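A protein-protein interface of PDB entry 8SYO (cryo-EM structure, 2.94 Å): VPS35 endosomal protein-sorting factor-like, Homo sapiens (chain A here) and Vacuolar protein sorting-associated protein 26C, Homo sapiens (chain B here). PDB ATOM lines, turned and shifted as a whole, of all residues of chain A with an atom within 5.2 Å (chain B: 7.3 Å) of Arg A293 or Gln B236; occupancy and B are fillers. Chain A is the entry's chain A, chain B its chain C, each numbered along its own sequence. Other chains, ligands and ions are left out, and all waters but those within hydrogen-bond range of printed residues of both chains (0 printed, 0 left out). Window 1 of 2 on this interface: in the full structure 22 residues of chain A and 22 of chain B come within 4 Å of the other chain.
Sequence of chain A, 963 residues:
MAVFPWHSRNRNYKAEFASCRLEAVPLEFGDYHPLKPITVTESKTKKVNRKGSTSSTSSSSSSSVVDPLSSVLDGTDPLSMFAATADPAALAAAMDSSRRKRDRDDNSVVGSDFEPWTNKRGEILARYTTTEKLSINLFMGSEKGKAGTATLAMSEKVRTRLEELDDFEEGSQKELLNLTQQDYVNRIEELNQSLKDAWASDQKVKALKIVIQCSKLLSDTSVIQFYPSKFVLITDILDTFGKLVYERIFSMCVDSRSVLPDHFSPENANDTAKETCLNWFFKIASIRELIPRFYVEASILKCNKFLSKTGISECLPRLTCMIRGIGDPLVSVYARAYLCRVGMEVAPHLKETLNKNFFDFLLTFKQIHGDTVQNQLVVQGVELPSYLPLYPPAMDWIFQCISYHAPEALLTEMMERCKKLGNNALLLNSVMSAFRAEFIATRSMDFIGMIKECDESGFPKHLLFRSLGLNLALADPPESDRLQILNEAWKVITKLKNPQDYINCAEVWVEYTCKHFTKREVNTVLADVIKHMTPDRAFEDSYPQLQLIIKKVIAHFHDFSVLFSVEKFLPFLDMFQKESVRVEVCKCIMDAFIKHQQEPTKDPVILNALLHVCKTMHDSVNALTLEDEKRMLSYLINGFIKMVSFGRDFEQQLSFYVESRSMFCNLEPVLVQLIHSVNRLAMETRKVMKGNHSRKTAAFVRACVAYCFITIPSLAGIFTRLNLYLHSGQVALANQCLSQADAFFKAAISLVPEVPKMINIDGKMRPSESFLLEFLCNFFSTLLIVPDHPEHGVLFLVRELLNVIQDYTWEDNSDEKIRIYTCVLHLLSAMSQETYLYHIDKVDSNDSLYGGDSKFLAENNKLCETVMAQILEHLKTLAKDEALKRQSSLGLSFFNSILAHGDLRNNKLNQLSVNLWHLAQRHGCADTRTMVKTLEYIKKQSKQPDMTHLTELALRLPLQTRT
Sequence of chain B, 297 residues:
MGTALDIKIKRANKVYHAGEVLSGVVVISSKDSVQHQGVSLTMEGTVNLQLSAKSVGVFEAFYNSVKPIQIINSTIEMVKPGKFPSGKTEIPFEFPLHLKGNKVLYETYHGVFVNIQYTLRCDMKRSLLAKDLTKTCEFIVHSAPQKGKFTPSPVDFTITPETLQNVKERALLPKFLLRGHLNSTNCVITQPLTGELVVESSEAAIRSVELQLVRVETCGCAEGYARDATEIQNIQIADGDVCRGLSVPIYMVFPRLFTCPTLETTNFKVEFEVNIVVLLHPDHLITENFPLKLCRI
Among the printed residues, pairs that only touch across the chains: Arg A288 with Asn B234 (3.1 Å), Arg A293 with Ile B235 (3.3 Å), Ile A291 with Asp B239 (3.3 Å), Leu A290 with Ile B237 (3.7 Å), Met A322 with Pro B249 (3.8 Å), Arg A288 with Ile B235 (3.9 Å) and Ala A285 with Ile B235 (3.96 Å).
O of Arg A288 lies within hydrogen-bond range of NH1 of Arg A293, 3.1 Å away. NE2 of Gln B236 is in hydrogen-bond range of OG of Ser B208. O of Ile A287 is in hydrogen-bond range of NH1 of Arg A293, at 3.1 Å. N of Ile B237 is in hydrogen-bond range of O of Val B209, 2.9 Å away. The side-chain amide nitrogen (NE2) of Gln B236 is in hydrogen-bond range of the backbone carbonyl oxygen (O) of Ala B238, 3.4 Å away. NE2 of Gln B236 sits at hydrogen-bond distance from OD1 of Asp B239, at 3.5 Å.
Of the printed residues of chain B, Ala A285 touches Ile B235. Of the printed residues of chain B, Arg A288 touches Glu B210, Asn B234, Ile B235 and Gln B236. Printed residues of chain B within 4 Å of Arg A293: Ile B235 (3.3 Å) and Gln B236 (2.9 Å). Of the printed residues of chain A, Ile B235 touches Ala A285 (3.96 Å), Arg A288 (3.9 Å) and Arg A293 (3.3 Å). Of the printed residues of chain A, Ile B237 touches Leu A290 (3.7 Å). The nearest residue of chain B that does not touch Arg A293 is Ile B237 (4.4 Å). The nearest printed residue of chain A that does not touch Gln B236 is Ile A287 (5.2 Å).
The backbone carbonyl oxygen of Gln B236 lies within hydrogen-bond range of the guanidinium group of Arg A293 (2.9 Å). OE1 of Glu B210 is in salt-bridge range of NH2 of Arg A288 (3.0 Å). N of Gln B236 lies within hydrogen-bond range of O of Arg A288 (2.9 Å). The side-chain carboxylate (OE1) of Glu A289 sits close to the side-chain amide oxygen (OE1) of Gln B236. N of Leu A290 is in hydrogen-bond range of OE1 of Gln B236 (3.2 Å).
Among the printed residues, 12 pairs touch across the chains.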
ATOM      1  N   ILE A 284     -18.988  20.519 -12.590  1.00  0.00           N
ATOM      2  CA  ILE A 284     -19.162  20.696 -14.027  1.00  0.00           C
ATOM      3  C   ILE A 284     -17.906  20.278 -14.785  1.00  0.00           C
ATOM      4  O   ILE A 284     -17.988  19.709 -15.879  1.00  0.00           O
ATOM      5  CB  ILE A 284     -19.572  22.146 -14.324  1.00  0.00           C
ATOM      6  CG1 ILE A 284     -21.013  22.346 -13.869  1.00  0.00           C
ATOM      7  CG2 ILE A 284     -19.433  22.456 -15.798  1.00  0.00           C
ATOM      8  CD1 ILE A 284     -21.450  23.759 -13.830  1.00  0.00           C
ATOM      9  N   ALA A 285     -16.729  20.537 -14.218  1.00  0.00           N
ATOM     10  CA  ALA A 285     -15.487  20.086 -14.827  1.00  0.00           C
ATOM     11  C   ALA A 285     -15.337  18.574 -14.805  1.00  0.00           C
ATOM     12  O   ALA A 285     -14.481  18.045 -15.518  1.00  0.00           O
ATOM     13  CB  ALA A 285     -14.293  20.731 -14.121  1.00  0.00           C
ATOM     14  N   ILE A 287     -17.595  16.516 -15.897  1.00  0.00           N
ATOM     15  CA  ILE A 287     -18.464  15.930 -16.910  1.00  0.00           C
ATOM     16  C   ILE A 287     -17.628  15.274 -18.000  1.00  0.00           C
ATOM     17  O   ILE A 287     -16.622  15.829 -18.462  1.00  0.00           O
ATOM     18  CB  ILE A 287     -19.405  16.997 -17.494  1.00  0.00           C
ATOM     19  CG1 ILE A 287     -20.243  17.626 -16.388  1.00  0.00           C
ATOM     20  CG2 ILE A 287     -20.314  16.386 -18.538  1.00  0.00           C
ATOM     21  CD1 ILE A 287     -21.096  18.769 -16.855  1.00  0.00           C
ATOM     22  N   ARG A 288     -18.046  14.080 -18.420  1.00  0.00           N
ATOM     23  CA  ARG A 288     -17.282  13.307 -19.394  1.00  0.00           C
ATOM     24  C   ARG A 288     -17.463  13.842 -20.808  1.00  0.00           C
ATOM     25  O   ARG A 288     -16.496  14.253 -21.457  1.00  0.00           O
ATOM     26  CB  ARG A 288     -17.693  11.835 -19.332  1.00  0.00           C
ATOM     27  CG  ARG A 288     -16.808  10.916 -20.149  1.00  0.00           C
ATOM     28  CD  ARG A 288     -17.562   9.700 -20.636  1.00  0.00           C
ATOM     29  NE  ARG A 288     -16.698   8.801 -21.392  1.00  0.00           N
ATOM     30  CZ  ARG A 288     -16.584   7.501 -21.158  1.00  0.00           C
ATOM     31  NH1 ARG A 288     -17.262   6.914 -20.186  1.00  0.00           N
ATOM     32  NH2 ARG A 288     -15.771   6.774 -21.917  1.00  0.00           N
ATOM     33  N   GLU A 289     -18.697  13.833 -21.304  1.00  0.00           N
ATOM     34  CA  GLU A 289     -18.951  14.214 -22.684  1.00  0.00           C
ATOM     35  C   GLU A 289     -18.607  15.682 -22.904  1.00  0.00           C
ATOM     36  O   GLU A 289     -18.863  16.533 -22.049  1.00  0.00           O
ATOM     37  CB  GLU A 289     -20.411  13.942 -23.039  1.00  0.00           C
ATOM     38  CG  GLU A 289     -20.794  12.471 -23.042  1.00  0.00           C
ATOM     39  CD  GLU A 289     -20.108  11.684 -24.138  1.00  0.00           C
ATOM     40  OE1 GLU A 289     -19.842  12.264 -25.213  1.00  0.00           O
ATOM     41  OE2 GLU A 289     -19.836  10.484 -23.929  1.00  0.00           O
ATOM     42  N   LEU A 290     -18.016  15.972 -24.063  1.00  0.00           N
ATOM     43  CA  LEU A 290     -17.443  17.292 -24.303  1.00  0.00           C
ATOM     44  C   LEU A 290     -18.518  18.362 -24.442  1.00  0.00           C
ATOM     45  O   LEU A 290     -18.425  19.430 -23.830  1.00  0.00           O
ATOM     46  CB  LEU A 290     -16.567  17.257 -25.552  1.00  0.00           C
ATOM     47  CG  LEU A 290     -16.057  18.614 -26.030  1.00  0.00           C
ATOM     48  CD1 LEU A 290     -14.874  19.048 -25.195  1.00  0.00           C
ATOM     49  CD2 LEU A 290     -15.684  18.546 -27.492  1.00  0.00           C
ATOM     50  N   ILE A 291     -19.528  18.102 -25.263  1.00  0.00           N
ATOM     51  CA  ILE A 291     -20.570  19.078 -25.570  1.00  0.00           C
ATOM     52  C   ILE A 291     -21.385  19.426 -24.324  1.00  0.00           C
ATOM     53  O   ILE A 291     -21.604  20.621 -24.057  1.00  0.00           O
ATOM     54  CB  ILE A 291     -21.455  18.573 -26.721  1.00  0.00           C
ATOM     55  CG1 ILE A 291     -20.671  18.625 -28.033  1.00  0.00           C
ATOM     56  CG2 ILE A 291     -22.729  19.379 -26.820  1.00  0.00           C
ATOM     57  CD1 ILE A 291     -21.099  17.598 -29.043  1.00  0.00           C
ATOM     58  N   PRO A 292     -21.865  18.448 -23.541  1.00  0.00           N
ATOM     59  CA  PRO A 292     -22.521  18.810 -22.275  1.00  0.00           C
ATOM     60  C   PRO A 292     -21.631  19.608 -21.349  1.00  0.00           C
ATOM     61  O   PRO A 292     -22.098  20.564 -20.720  1.00  0.00           O
ATOM     62  CB  PRO A 292     -22.875  17.449 -21.664  1.00  0.00           C
ATOM     63  CG  PRO A 292     -22.911  16.531 -22.784  1.00  0.00           C
ATOM     64  CD  PRO A 292     -21.893  16.991 -23.753  1.00  0.00           C
ATOM     65  N   ARG A 293     -20.352  19.242 -21.250  1.00  0.00           N
ATOM     66  CA  ARG A 293     -19.444  19.971 -20.375  1.00  0.00           C
ATOM     67  C   ARG A 293     -19.324  21.421 -20.810  1.00  0.00           C
ATOM     68  O   ARG A 293     -19.444  22.340 -19.992  1.00  0.00           O
ATOM     69  CB  ARG A 293     -18.074  19.302 -20.363  1.00  0.00           C
ATOM     70  CG  ARG A 293     -17.065  20.005 -19.490  1.00  0.00           C
ATOM     71  CD  ARG A 293     -15.936  19.078 -19.111  1.00  0.00           C
ATOM     72  NE  ARG A 293     -14.861  19.118 -20.091  1.00  0.00           N
ATOM     73  CZ  ARG A 293     -14.604  18.151 -20.958  1.00  0.00           C
ATOM     74  NH1 ARG A 293     -15.319  17.040 -20.985  1.00  0.00           N
ATOM     75  NH2 ARG A 293     -13.598  18.297 -21.813  1.00  0.00           N
ATOM     76  N   PHE A 294     -19.118  21.645 -22.109  1.00  0.00           N
ATOM     77  CA  PHE A 294     -18.989  23.008 -22.607  1.00  0.00           C
ATOM     78  C   PHE A 294     -20.254  23.806 -22.339  1.00  0.00           C
ATOM     79  O   PHE A 294     -20.191  24.946 -21.866  1.00  0.00           O
ATOM     80  CB  PHE A 294     -18.680  23.015 -24.100  1.00  0.00           C
ATOM     81  CG  PHE A 294     -19.108  24.278 -24.783  1.00  0.00           C
ATOM     82  CD1 PHE A 294     -18.371  25.437 -24.641  1.00  0.00           C
ATOM     83  CD2 PHE A 294     -20.263  24.318 -25.537  1.00  0.00           C
ATOM     84  CE1 PHE A 294     -18.769  26.602 -25.249  1.00  0.00           C
ATOM     85  CE2 PHE A 294     -20.666  25.485 -26.143  1.00  0.00           C
ATOM     86  CZ  PHE A 294     -19.916  26.626 -26.001  1.00  0.00           C
ATOM     87  N   TYR A 295     -21.416  23.228 -22.645  1.00  0.00           N
ATOM     88  CA  TYR A 295     -22.658  23.979 -22.502  1.00  0.00           C
ATOM     89  C   TYR A 295     -22.933  24.316 -21.043  1.00  0.00           C
ATOM     90  O   TYR A 295     -23.239  25.469 -20.708  1.00  0.00           O
ATOM     91  CB  TYR A 295     -23.818  23.192 -23.107  1.00  0.00           C
ATOM     92  CG  TYR A 295     -23.990  23.429 -24.586  1.00  0.00           C
ATOM     93  CD1 TYR A 295     -24.281  24.689 -25.075  1.00  0.00           C
ATOM     94  CD2 TYR A 295     -23.849  22.396 -25.492  1.00  0.00           C
ATOM     95  CE1 TYR A 295     -24.436  24.911 -26.423  1.00  0.00           C
ATOM     96  CE2 TYR A 295     -24.001  22.609 -26.841  1.00  0.00           C
ATOM     97  CZ  TYR A 295     -24.295  23.865 -27.301  1.00  0.00           C
ATOM     98  OH  TYR A 295     -24.448  24.077 -28.649  1.00  0.00           O
ATOM     99  N   VAL A 296     -22.802  23.331 -20.153  1.00  0.00           N
ATOM    100  CA  VAL A 296     -23.101  23.560 -18.744  1.00  0.00           C
ATOM    101  C   VAL A 296     -22.101  24.535 -18.136  1.00  0.00           C
ATOM    102  O   VAL A 296     -22.456  25.355 -17.282  1.00  0.00           O
ATOM    103  CB  VAL A 296     -23.138  22.222 -17.984  1.00  0.00           C
ATOM    104  CG1 VAL A 296     -23.422  22.455 -16.524  1.00  0.00           C
ATOM    105  CG2 VAL A 296     -24.204  21.320 -18.567  1.00  0.00           C
ATOM    106  N   GLU A 297     -20.839  24.479 -18.572  1.00  0.00           N
ATOM    107  CA  GLU A 297     -19.835  25.370 -18.003  1.00  0.00           C
ATOM    108  C   GLU A 297     -19.999  26.793 -18.517  1.00  0.00           C
ATOM    109  O   GLU A 297     -19.823  27.754 -17.759  1.00  0.00           O
ATOM    110  CB  GLU A 297     -18.437  24.842 -18.308  1.00  0.00           C
ATOM    111  CG  GLU A 297     -17.335  25.580 -17.587  1.00  0.00           C
ATOM    112  CD  GLU A 297     -15.988  24.917 -17.764  1.00  0.00           C
ATOM    113  OE1 GLU A 297     -15.910  23.916 -18.504  1.00  0.00           O
ATOM    114  OE2 GLU A 297     -15.010  25.388 -17.148  1.00  0.00           O
ATOM    115  N   ALA A 298     -20.327  26.954 -19.800  1.00  0.00           N
ATOM    116  CA  ALA A 298     -20.550  28.290 -20.338  1.00  0.00           C
ATOM    117  C   ALA A 298     -21.845  28.885 -19.804  1.00  0.00           C
ATOM    118  O   ALA A 298     -22.013  30.109 -19.795  1.00  0.00           O
ATOM    119  CB  ALA A 298     -20.566  28.249 -21.863  1.00  0.00           C
ATOM    120  N   MET A 322     -11.888  24.993 -26.494  1.00  0.00           N
ATOM    121  CA  MET A 322     -12.555  23.717 -26.260  1.00  0.00           C
ATOM    122  C   MET A 322     -13.517  23.368 -27.380  1.00  0.00           C
ATOM    123  O   MET A 322     -13.721  22.187 -27.678  1.00  0.00           O
ATOM    124  CB  MET A 322     -13.305  23.770 -24.929  1.00  0.00           C
ATOM    125  CG  MET A 322     -13.947  22.469 -24.509  1.00  0.00           C
ATOM    126  SD  MET A 322     -14.796  22.630 -22.931  1.00  0.00           S
ATOM    127  CE  MET A 322     -13.402  22.749 -21.814  1.00  0.00           C
ATOM    128  N   ARG B 207     -13.953   8.797 -33.826  1.00  0.00           N
ATOM    129  CA  ARG B 207     -15.218   8.918 -33.113  1.00  0.00           C
ATOM    130  C   ARG B 207     -15.066   9.750 -31.847  1.00  0.00           C
ATOM    131  O   ARG B 207     -15.918  10.596 -31.552  1.00  0.00           O
ATOM    132  CB  ARG B 207     -15.764   7.531 -32.781  1.00  0.00           C
ATOM    133  CG  ARG B 207     -17.161   7.545 -32.191  1.00  0.00           C
ATOM    134  CD  ARG B 207     -17.590   6.155 -31.763  1.00  0.00           C
ATOM    135  NE  ARG B 207     -17.795   5.271 -32.903  1.00  0.00           N
ATOM    136  CZ  ARG B 207     -18.015   3.967 -32.807  1.00  0.00           C
ATOM    137  NH1 ARG B 207     -18.062   3.361 -31.633  1.00  0.00           N
ATOM    138  NH2 ARG B 207     -18.193   3.256 -33.916  1.00  0.00           N
ATOM    139  N   SER B 208     -13.992   9.533 -31.090  1.00  0.00           N
ATOM    140  CA  SER B 208     -13.825  10.222 -29.818  1.00  0.00           C
ATOM    141  C   SER B 208     -12.385  10.096 -29.348  1.00  0.00           C
ATOM    142  O   SER B 208     -11.771   9.037 -29.490  1.00  0.00           O
ATOM    143  CB  SER B 208     -14.771   9.655 -28.755  1.00  0.00           C
ATOM    144  OG  SER B 208     -14.586  10.304 -27.510  1.00  0.00           O
ATOM    145  N   VAL B 209     -11.861  11.185 -28.792  1.00  0.00           N
ATOM    146  CA  VAL B 209     -10.578  11.203 -28.100  1.00  0.00           C
ATOM    147  C   VAL B 209     -10.833  11.722 -26.694  1.00  0.00           C
ATOM    148  O   VAL B 209     -11.353  12.833 -26.527  1.00  0.00           O
ATOM    149  CB  VAL B 209      -9.537  12.078 -28.812  1.00  0.00           C
ATOM    150  CG1 VAL B 209      -8.174  11.879 -28.182  1.00  0.00           C
ATOM    151  CG2 VAL B 209      -9.493  11.760 -30.288  1.00  0.00           C
ATOM    152  N   GLU B 210     -10.468  10.928 -25.689  1.00  0.00           N
ATOM    153  CA  GLU B 210     -10.772  11.253 -24.307  1.00  0.00           C
ATOM    154  C   GLU B 210      -9.570  10.970 -23.420  1.00  0.00           C
ATOM    155  O   GLU B 210      -8.770  10.074 -23.694  1.00  0.00           O
ATOM    156  CB  GLU B 210     -11.996  10.471 -23.810  1.00  0.00           C
ATOM    157  CG  GLU B 210     -11.795   8.974 -23.741  1.00  0.00           C
ATOM    158  CD  GLU B 210     -13.044   8.234 -23.311  1.00  0.00           C
ATOM    159  OE1 GLU B 210     -14.081   8.894 -23.088  1.00  0.00           O
ATOM    160  OE2 GLU B 210     -12.990   6.991 -23.198  1.00  0.00           O
ATOM    161  N   LEU B 211      -9.453  11.757 -22.357  1.00  0.00           N
ATOM    162  CA  LEU B 211      -8.448  11.556 -21.327  1.00  0.00           C
ATOM    163  C   LEU B 211      -9.001  10.643 -20.244  1.00  0.00           C
ATOM    164  O   LEU B 211     -10.207  10.613 -19.987  1.00  0.00           O
ATOM    165  CB  LEU B 211      -8.025  12.892 -20.720  1.00  0.00           C
ATOM    166  CG  LEU B 211      -7.304  13.877 -21.638  1.00  0.00           C
ATOM    167  CD1 LEU B 211      -7.431  15.277 -21.089  1.00  0.00           C
ATOM    168  CD2 LEU B 211      -5.853  13.500 -21.751  1.00  0.00           C
ATOM    169  N   GLN B 212      -8.108   9.893 -19.608  1.00  0.00           N
ATOM    170  CA  GLN B 212      -8.505   8.874 -18.639  1.00  0.00           C
ATOM    171  C   GLN B 212      -7.485   8.875 -17.508  1.00  0.00           C
ATOM    172  O   GLN B 212      -6.419   8.265 -17.626  1.00  0.00           O
ATOM    173  CB  GLN B 212      -8.605   7.510 -19.306  1.00  0.00           C
ATOM    174  CG  GLN B 212      -8.909   6.368 -18.366  1.00  0.00           C
ATOM    175  CD  GLN B 212      -9.073   5.055 -19.097  1.00  0.00           C
ATOM    176  OE1 GLN B 212      -9.471   5.026 -20.260  1.00  0.00           O
ATOM    177  NE2 GLN B 212      -8.765   3.959 -18.420  1.00  0.00           N
ATOM    178  N   ASN B 234     -13.148   9.976 -16.729  1.00  0.00           N
ATOM    179  CA  ASN B 234     -12.898  10.130 -18.152  1.00  0.00           C
ATOM    180  C   ASN B 234     -13.404  11.495 -18.585  1.00  0.00           C
ATOM    181  O   ASN B 234     -14.524  11.883 -18.240  1.00  0.00           O
ATOM    182  CB  ASN B 234     -13.583   9.026 -18.956  1.00  0.00           C
ATOM    183  CG  ASN B 234     -12.906   7.688 -18.796  1.00  0.00           C
ATOM    184  OD1 ASN B 234     -13.148   6.969 -17.830  1.00  0.00           O
ATOM    185  ND2 ASN B 234     -12.048   7.343 -19.747  1.00  0.00           N
ATOM    186  N   ILE B 235     -12.573  12.230 -19.317  1.00  0.00           N
ATOM    187  CA  ILE B 235     -12.921  13.554 -19.815  1.00  0.00           C
ATOM    188  C   ILE B 235     -12.673  13.567 -21.317  1.00  0.00           C
ATOM    189  O   ILE B 235     -11.524  13.606 -21.768  1.00  0.00           O
ATOM    190  CB  ILE B 235     -12.150  14.671 -19.107  1.00  0.00           C
ATOM    191  CG1 ILE B 235     -12.524  14.698 -17.625  1.00  0.00           C
ATOM    192  CG2 ILE B 235     -12.405  16.004 -19.758  1.00  0.00           C
ATOM    193  CD1 ILE B 235     -11.653  15.579 -16.789  1.00  0.00           C
ATOM    194  N   GLN B 236     -13.752  13.524 -22.093  1.00  0.00           N
ATOM    195  CA  GLN B 236     -13.650  13.574 -23.541  1.00  0.00           C
ATOM    196  C   GLN B 236     -13.226  14.963 -23.993  1.00  0.00           C
ATOM    197  O   GLN B 236     -13.755  15.974 -23.525  1.00  0.00           O
ATOM    198  CB  GLN B 236     -14.989  13.202 -24.173  1.00  0.00           C
ATOM    199  CG  GLN B 236     -14.946  12.966 -25.663  1.00  0.00           C
ATOM    200  CD  GLN B 236     -16.331  12.873 -26.262  1.00  0.00           C
ATOM    201  OE1 GLN B 236     -17.300  13.348 -25.677  1.00  0.00           O
ATOM    202  NE2 GLN B 236     -16.434  12.251 -27.426  1.00  0.00           N
ATOM    203  N   ILE B 237     -12.264  15.010 -24.909  1.00  0.00           N
ATOM    204  CA  ILE B 237     -11.779  16.275 -25.439  1.00  0.00           C
ATOM    205  C   ILE B 237     -12.067  16.452 -26.922  1.00  0.00           C
ATOM    206  O   ILE B 237     -12.117  17.601 -27.391  1.00  0.00           O
ATOM    207  CB  ILE B 237     -10.270  16.450 -25.170  1.00  0.00           C
ATOM    208  CG1 ILE B 237      -9.491  15.271 -25.745  1.00  0.00           C
ATOM    209  CG2 ILE B 237     -10.010  16.592 -23.685  1.00  0.00           C
ATOM    210  CD1 ILE B 237      -8.013  15.501 -25.832  1.00  0.00           C
ATOM    211  N   ALA B 238     -12.253  15.380 -27.687  1.00  0.00           N
ATOM    212  CA  ALA B 238     -12.564  15.487 -29.107  1.00  0.00           C
ATOM    213  C   ALA B 238     -13.749  14.589 -29.417  1.00  0.00           C
ATOM    214  O   ALA B 238     -13.689  13.382 -29.175  1.00  0.00           O
ATOM    215  CB  ALA B 238     -11.358  15.104 -29.968  1.00  0.00           C
ATOM    216  N   ASP B 239     -14.815  15.175 -29.955  1.00  0.00           N
ATOM    217  CA  ASP B 239     -16.026  14.451 -30.312  1.00  0.00           C
ATOM    218  C   ASP B 239     -16.256  14.574 -31.809  1.00  0.00           C
ATOM    219  O   ASP B 239     -16.278  15.686 -32.347  1.00  0.00           O
ATOM    220  CB  ASP B 239     -17.234  14.988 -29.546  1.00  0.00           C
ATOM    221  CG  ASP B 239     -18.481  14.156 -29.764  1.00  0.00           C
ATOM    222  OD1 ASP B 239     -18.357  13.003 -30.228  1.00  0.00           O
ATOM    223  OD2 ASP B 239     -19.588  14.654 -29.469  1.00  0.00           O
ATOM    224  N   GLY B 240     -16.430  13.438 -32.477  1.00  0.00           N
ATOM    225  CA  GLY B 240     -16.619  13.435 -33.911  1.00  0.00           C
ATOM    226  C   GLY B 240     -15.314  13.598 -34.664  1.00  0.00           C
ATOM    227  O   GLY B 240     -14.228  13.699 -34.093  1.00  0.00           O
ATOM    228  N   PRO B 249      -7.460  21.258 -27.678  1.00  0.00           N
ATOM    229  CA  PRO B 249      -6.813  21.533 -26.392  1.00  0.00           C
ATOM    230  C   PRO B 249      -7.062  20.457 -25.349  1.00  0.00           C
ATOM    231  O   PRO B 249      -8.200  20.233 -24.927  1.00  0.00           O
ATOM    232  CB  PRO B 249      -7.436  22.867 -25.975  1.00  0.00           C
ATOM    233  CG  PRO B 249      -8.778  22.849 -26.587  1.00  0.00           C
ATOM    234  CD  PRO B 249      -8.678  22.061 -27.866  1.00  0.00           C
ATOM    235  N   TYR B 251      -7.344  19.567 -21.860  1.00  0.00           N
ATOM    236  CA  TYR B 251      -7.593  20.283 -20.615  1.00  0.00           C
ATOM    237  C   TYR B 251      -8.221  19.312 -19.636  1.00  0.00           C
ATOM    238  O   TYR B 251      -9.194  18.633 -19.978  1.00  0.00           O
ATOM    239  CB  TYR B 251      -8.514  21.476 -20.827  1.00  0.00           C
ATOM    240  CG  TYR B 251      -8.605  22.368 -19.619  1.00  0.00           C
ATOM    241  CD1 TYR B 251      -9.794  22.504 -18.921  1.00  0.00           C
ATOM    242  CD2 TYR B 251      -7.512  23.098 -19.193  1.00  0.00           C
ATOM    243  CE1 TYR B 251      -9.881  23.320 -17.816  1.00  0.00           C
ATOM    244  CE2 TYR B 251      -7.594  23.924 -18.103  1.00  0.00           C
ATOM    245  CZ  TYR B 251      -8.776  24.030 -17.412  1.00  0.00           C
ATOM    246  OH  TYR B 251      -8.857  24.853 -16.315  1.00  0.00           O
ATOM    247  N   MET B 252      -7.677  19.243 -18.428  1.00  0.00           N
ATOM    248  CA  MET B 252      -8.221  18.338 -17.429  1.00  0.00           C
ATOM    249  C   MET B 252      -8.092  18.945 -16.043  1.00  0.00           C
ATOM    250  O   MET B 252      -7.003  19.365 -15.646  1.00  0.00           O
ATOM    251  CB  MET B 252      -7.514  16.986 -17.478  1.00  0.00           C
ATOM    252  CG  MET B 252      -8.208  15.940 -16.670  1.00  0.00           C
ATOM    253  SD  MET B 252      -7.560  14.295 -16.936  1.00  0.00           S
ATOM    254  CE  MET B 252      -8.743  13.383 -15.967  1.00  0.00           C
